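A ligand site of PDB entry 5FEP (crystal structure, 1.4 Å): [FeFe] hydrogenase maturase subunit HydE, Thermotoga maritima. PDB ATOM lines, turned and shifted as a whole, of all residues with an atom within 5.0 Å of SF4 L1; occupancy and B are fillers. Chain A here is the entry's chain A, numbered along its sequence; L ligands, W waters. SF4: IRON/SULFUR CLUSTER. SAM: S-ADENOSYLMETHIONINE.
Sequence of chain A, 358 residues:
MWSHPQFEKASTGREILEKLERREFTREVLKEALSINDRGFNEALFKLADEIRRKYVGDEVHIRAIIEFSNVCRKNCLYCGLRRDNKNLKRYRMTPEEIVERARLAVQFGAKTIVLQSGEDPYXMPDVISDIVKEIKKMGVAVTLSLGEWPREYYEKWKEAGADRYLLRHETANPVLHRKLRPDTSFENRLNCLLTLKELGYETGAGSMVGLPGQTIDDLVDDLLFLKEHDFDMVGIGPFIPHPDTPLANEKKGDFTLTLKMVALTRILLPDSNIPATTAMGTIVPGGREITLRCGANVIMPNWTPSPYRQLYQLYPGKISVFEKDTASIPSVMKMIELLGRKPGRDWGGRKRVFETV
An iron atom (FE2) of SF4 L1 is bound by the side-chain sulfur (SG) of Cys 73.
N of Cys 77 lies close to S4 of SF4 L1.
An iron atom (FE3) of SF4 L1 is bound by the side-chain sulfur (SG) of Cys 77 (2.3 Å).
An iron atom (FE1) of SF4 L1 is bound by the side-chain sulfur (SG) of Cys 80 (2.3 Å).
The backbone carbonyl oxygen (O) of Tyr 79 sits at hydrogen-bond distance from a nitrogen (N6) of SAM L2 (2.8 Å).
A nitrogen (N) of SAM L2 lies close to the backbone carbonyl oxygen (O) of Ser 118.
An iron atom (FE4) of SF4 L1 is bound by an oxygen (OXT) of SAM L2 (2.2 Å).
SG of Cys 73 sits close to N of Lys 75.
SG of Cys 73 sits close to N of Glu 120, at 3.3 Å.
The side-chain sulfur (SG) of Cys 77 lies close to the side-chain hydroxyl (OH) of Tyr 79 (3.8 Å).
NE of Arg 182 lies close to SG of Cys 77, 3.6 Å away.
The side-chain sulfur (SG) of Cys 80 lies close to the backbone NH (N) of Leu 82, 3.4 Å away.
The side-chain hydroxyl (OH) of Tyr 79 is in hydrogen-bond range of the guanidinium group (NE) of Arg 182 (3.0 Å).
NH2 of Arg 83 sits at hydrogen-bond distance from O of Asn 76, 2.9 Å away.
OE1 of Glu 120 is in salt-bridge range of NZ of Lys 75 (2.7 Å).
Residues that only touch SF4 L1: Lys 75, Tyr 79, Arg 83 and Gly 119.
Within 4 Å of SF4 L1: Cys 73, Lys 75, Cys 77, Tyr 79, Cys 80, Arg 83 and Gly 119.
The nearest printed residue that does not touch SF4 L1 is Glu 120 (4.04 Å).
Water W1 lies within hydrogen-bond range of OH of Tyr 79 (2.8 Å), NE of Arg 182 (3.1 Å) and S2 of SF4 L1 (3.2 Å).
Water W2 lies within hydrogen-bond range of the side-chain carboxylate (OE2) of Glu 120 (2.6 Å), a sulfur (S1) of SF4 L1 (3.3 Å) and the guanidinium group (NH2) of Arg 182 (3.4 Å).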
ATOM      1  N   CYS A  73     -28.916 -26.560 -19.331  1.00  0.00           N
ATOM      2  CA  CYS A  73     -27.788 -26.450 -20.225  1.00  0.00           C
ATOM      3  C   CYS A  73     -27.134 -25.076 -20.209  1.00  0.00           C
ATOM      4  O   CYS A  73     -27.850 -24.068 -20.241  1.00  0.00           O
ATOM      5  CB  CYS A  73     -28.079 -26.890 -21.678  1.00  0.00           C
ATOM      6  SG  CYS A  73     -26.653 -27.169 -22.704  1.00  0.00           S
ATOM      7  N   LYS A  75     -24.997 -24.214 -22.785  1.00  0.00           N
ATOM      8  CA  LYS A  75     -24.790 -23.883 -24.156  1.00  0.00           C
ATOM      9  C   LYS A  75     -26.075 -23.391 -24.814  1.00  0.00           C
ATOM     10  O   LYS A  75     -27.155 -23.484 -24.257  1.00  0.00           O
ATOM     11  CB  LYS A  75     -24.192 -25.076 -24.942  1.00  0.00           C
ATOM     12  CG  LYS A  75     -22.720 -25.280 -24.701  1.00  0.00           C
ATOM     13  CD  LYS A  75     -22.107 -26.317 -25.594  1.00  0.00           C
ATOM     14  CE  LYS A  75     -20.605 -26.360 -25.645  1.00  0.00           C
ATOM     15  NZ  LYS A  75     -19.881 -26.407 -24.333  1.00  0.00           N
ATOM     16  N   ASN A  76     -25.918 -22.815 -26.027  1.00  0.00           N
ATOM     17  CA  ASN A  76     -26.994 -22.080 -26.671  1.00  0.00           C
ATOM     18  C   ASN A  76     -27.164 -22.493 -28.126  1.00  0.00           C
ATOM     19  O   ASN A  76     -27.460 -21.704 -29.018  1.00  0.00           O
ATOM     20  CB  ASN A  76     -26.715 -20.565 -26.590  1.00  0.00           C
ATOM     21  CG  ASN A  76     -27.976 -19.741 -26.528  1.00  0.00           C
ATOM     22  OD1 ASN A  76     -29.020 -20.151 -26.115  1.00  0.00           O
ATOM     23  ND2 ASN A  76     -27.823 -18.426 -26.978  1.00  0.00           N
ATOM     24  N   CYS A  77     -27.032 -23.815 -28.384  1.00  0.00           N
ATOM     25  CA  CYS A  77     -27.123 -24.327 -29.752  1.00  0.00           C
ATOM     26  C   CYS A  77     -28.445 -23.869 -30.388  1.00  0.00           C
ATOM     27  O   CYS A  77     -29.501 -23.902 -29.788  1.00  0.00           O
ATOM     28  CB  CYS A  77     -27.031 -25.868 -29.761  1.00  0.00           C
ATOM     29  SG  CYS A  77     -25.569 -26.534 -28.911  1.00  0.00           S
ATOM     30  N   TYR A  79     -30.386 -24.894 -32.696  1.00  0.00           N
ATOM     31  CA  TYR A  79     -31.443 -25.921 -33.025  1.00  0.00           C
ATOM     32  C   TYR A  79     -32.160 -26.498 -31.816  1.00  0.00           C
ATOM     33  O   TYR A  79     -33.255 -27.071 -31.988  1.00  0.00           O
ATOM     34  CB  TYR A  79     -30.843 -27.070 -33.837  1.00  0.00           C
ATOM     35  CG  TYR A  79     -29.505 -27.570 -33.303  1.00  0.00           C
ATOM     36  CD1 TYR A  79     -29.492 -28.476 -32.220  1.00  0.00           C
ATOM     37  CD2 TYR A  79     -28.274 -27.199 -33.835  1.00  0.00           C
ATOM     38  CE1 TYR A  79     -28.314 -28.940 -31.737  1.00  0.00           C
ATOM     39  CE2 TYR A  79     -27.097 -27.674 -33.326  1.00  0.00           C
ATOM     40  CZ  TYR A  79     -27.098 -28.550 -32.262  1.00  0.00           C
ATOM     41  OH  TYR A  79     -25.898 -28.987 -31.788  1.00  0.00           O
ATOM     42  N   CYS A  80     -31.592 -26.344 -30.606  1.00  0.00           N
ATOM     43  CA  CYS A  80     -32.037 -27.164 -29.490  1.00  0.00           C
ATOM     44  C   CYS A  80     -32.997 -26.511 -28.552  1.00  0.00           C
ATOM     45  O   CYS A  80     -32.678 -25.369 -28.059  1.00  0.00           O
ATOM     46  CB  CYS A  80     -30.798 -27.567 -28.713  1.00  0.00           C
ATOM     47  SG  CYS A  80     -31.167 -28.775 -27.350  1.00  0.00           S
ATOM     48  N   LEU A  82     -33.391 -27.096 -25.457  1.00  0.00           N
ATOM     49  CA  LEU A  82     -32.769 -26.947 -24.129  1.00  0.00           C
ATOM     50  C   LEU A  82     -31.746 -25.787 -24.085  1.00  0.00           C
ATOM     51  O   LEU A  82     -31.161 -25.540 -23.011  1.00  0.00           O
ATOM     52  CB  LEU A  82     -32.042 -28.245 -23.681  1.00  0.00           C
ATOM     53  CG  LEU A  82     -32.916 -29.500 -23.617  1.00  0.00           C
ATOM     54  CD1 LEU A  82     -32.105 -30.584 -22.821  1.00  0.00           C
ATOM     55  CD2 LEU A  82     -34.343 -29.396 -23.170  1.00  0.00           C
ATOM     56  N   ARG A  83     -31.549 -25.077 -25.198  1.00  0.00           N
ATOM     57  CA  ARG A  83     -30.577 -23.965 -25.225  1.00  0.00           C
ATOM     58  C   ARG A  83     -30.808 -22.978 -24.053  1.00  0.00           C
ATOM     59  O   ARG A  83     -31.900 -22.722 -23.646  1.00  0.00           O
ATOM     60  CB  ARG A  83     -30.601 -23.240 -26.597  1.00  0.00           C
ATOM     61  CG  ARG A  83     -31.940 -22.506 -26.866  1.00  0.00           C
ATOM     62  CD  ARG A  83     -32.122 -22.177 -28.345  1.00  0.00           C
ATOM     63  NE  ARG A  83     -30.913 -21.519 -28.886  1.00  0.00           N
ATOM     64  CZ  ARG A  83     -30.714 -20.172 -28.954  1.00  0.00           C
ATOM     65  NH1 ARG A  83     -31.637 -19.352 -28.497  1.00  0.00           N
ATOM     66  NH2 ARG A  83     -29.584 -19.742 -29.453  1.00  0.00           N
ATOM     67  N   SER A 118     -27.891 -35.702 -20.611  1.00  0.00           N
ATOM     68  CA  SER A 118     -28.366 -34.409 -20.044  1.00  0.00           C
ATOM     69  C   SER A 118     -27.907 -33.262 -20.931  1.00  0.00           C
ATOM     70  O   SER A 118     -27.107 -33.406 -21.775  1.00  0.00           O
ATOM     71  CB  SER A 118     -27.732 -34.204 -18.691  1.00  0.00           C
ATOM     72  OG  SER A 118     -26.309 -34.128 -18.749  1.00  0.00           O
ATOM     73  N   GLY A 119     -28.521 -32.108 -20.659  1.00  0.00           N
ATOM     74  CA  GLY A 119     -27.859 -30.879 -21.162  1.00  0.00           C
ATOM     75  C   GLY A 119     -26.502 -30.782 -20.496  1.00  0.00           C
ATOM     76  O   GLY A 119     -26.160 -31.533 -19.561  1.00  0.00           O
ATOM     77  N   GLU A 120     -25.728 -29.814 -20.965  1.00  0.00           N
ATOM     78  CA  GLU A 120     -24.435 -29.497 -20.309  1.00  0.00           C
ATOM     79  C   GLU A 120     -24.696 -28.786 -19.005  1.00  0.00           C
ATOM     80  O   GLU A 120     -24.634 -27.526 -18.937  1.00  0.00           O
ATOM     81  CB  GLU A 120     -23.489 -28.725 -21.214  1.00  0.00           C
ATOM     82  CG  GLU A 120     -23.011 -29.554 -22.399  1.00  0.00           C
ATOM     83  CD  GLU A 120     -21.803 -28.946 -23.100  1.00  0.00           C
ATOM     84  OE1 GLU A 120     -21.242 -27.938 -22.601  1.00  0.00           O
ATOM     85  OE2 GLU A 120     -21.376 -29.454 -24.125  1.00  0.00           O
ATOM     86  N   ARG A 182     -23.609 -23.655 -33.288  1.00  0.00           N
ATOM     87  CA  ARG A 182     -23.119 -23.979 -31.938  1.00  0.00           C
ATOM     88  C   ARG A 182     -22.122 -22.898 -31.489  1.00  0.00           C
ATOM     89  O   ARG A 182     -20.894 -23.125 -31.471  1.00  0.00           O
ATOM     90  CB  ARG A 182     -22.547 -25.372 -31.938  1.00  0.00           C
ATOM     91  CG  ARG A 182     -23.539 -26.398 -32.541  1.00  0.00           C
ATOM     92  CD  ARG A 182     -23.049 -27.860 -32.391  1.00  0.00           C
ATOM     93  NE  ARG A 182     -23.141 -28.200 -30.961  1.00  0.00           N
ATOM     94  CZ  ARG A 182     -22.111 -28.417 -30.157  1.00  0.00           C
ATOM     95  NH1 ARG A 182     -20.898 -28.540 -30.582  1.00  0.00           N
ATOM     96  NH2 ARG A 182     -22.357 -28.546 -28.855  1.00  0.00           N
HETATM   97 FE1  SF4 L   1     -28.997 -28.870 -26.536  1.00  0.00          FE
HETATM   98 FE2  SF4 L   1     -27.217 -28.037 -24.682  1.00  0.00          FE
HETATM   99 FE3  SF4 L   1     -26.557 -27.913 -27.339  1.00  0.00          FE
HETATM  100 FE4  SF4 L   1     -26.710 -30.479 -26.043  1.00  0.00          FE
HETATM  101  S1  SF4 L   1     -25.239 -28.675 -25.652  1.00  0.00           S
HETATM  102  S2  SF4 L   1     -27.605 -29.790 -28.124  1.00  0.00           S
HETATM  103  S3  SF4 L   1     -28.496 -29.940 -24.622  1.00  0.00           S
HETATM  104  S4  SF4 L   1     -28.166 -26.726 -26.239  1.00  0.00           S
HETATM  105  N   SAM L   2     -25.895 -31.989 -24.467  1.00  0.00           N
HETATM  106  CA  SAM L   2     -25.298 -33.252 -24.965  1.00  0.00           C
HETATM  107  C   SAM L   2     -24.819 -32.920 -26.362  1.00  0.00           C
HETATM  108  O   SAM L   2     -24.065 -33.762 -26.911  1.00  0.00           O
HETATM  109  OXT SAM L   2     -25.340 -31.876 -26.959  1.00  0.00           O
HETATM  110  CB  SAM L   2     -26.393 -34.358 -24.991  1.00  0.00           C
HETATM  111  CG  SAM L   2     -27.862 -33.810 -25.043  1.00  0.00           C
HETATM  112  SD  SAM L   2     -28.403 -33.156 -26.756  1.00  0.00           S
HETATM  113  CE  SAM L   2     -29.967 -32.570 -26.604  1.00  0.00           C
HETATM  114  C5' SAM L   2     -28.528 -34.720 -27.766  1.00  0.00           C
HETATM  115  C4' SAM L   2     -28.671 -34.518 -29.275  1.00  0.00           C
HETATM  116  O4' SAM L   2     -29.936 -33.998 -29.570  1.00  0.00           O
HETATM  117  C3' SAM L   2     -27.681 -33.561 -29.949  1.00  0.00           C
HETATM  118  O3' SAM L   2     -26.466 -34.233 -30.165  1.00  0.00           O
HETATM  119  C2' SAM L   2     -28.442 -33.213 -31.279  1.00  0.00           C
HETATM  120  O2' SAM L   2     -28.042 -33.950 -32.382  1.00  0.00           O
HETATM  121  C1' SAM L   2     -29.945 -33.649 -30.904  1.00  0.00           C
HETATM  122  N9  SAM L   2     -30.907 -32.585 -31.139  1.00  0.00           N
HETATM  123  C8  SAM L   2     -30.909 -31.403 -30.445  1.00  0.00           C
HETATM  124  N7  SAM L   2     -31.868 -30.591 -30.953  1.00  0.00           N
HETATM  125  C5  SAM L   2     -32.455 -31.235 -31.968  1.00  0.00           C
HETATM  126  C6  SAM L   2     -33.411 -30.886 -32.817  1.00  0.00           C
HETATM  127  N6  SAM L   2     -34.050 -29.675 -32.755  1.00  0.00           N
HETATM  128  N1  SAM L   2     -33.849 -31.748 -33.715  1.00  0.00           N
HETATM  129  C2  SAM L   2     -33.241 -33.029 -33.819  1.00  0.00           C
HETATM  130  N3  SAM L   2     -32.280 -33.344 -32.946  1.00  0.00           N
HETATM  131  C4  SAM L   2     -31.848 -32.455 -32.060  1.00  0.00           C
HETATM  132  O   HOH W   1     -24.881 -30.419 -29.644  1.00  0.00           O
HETATM  133  O   HOH W   2     -22.606 -30.542 -26.165  1.00  0.00           O
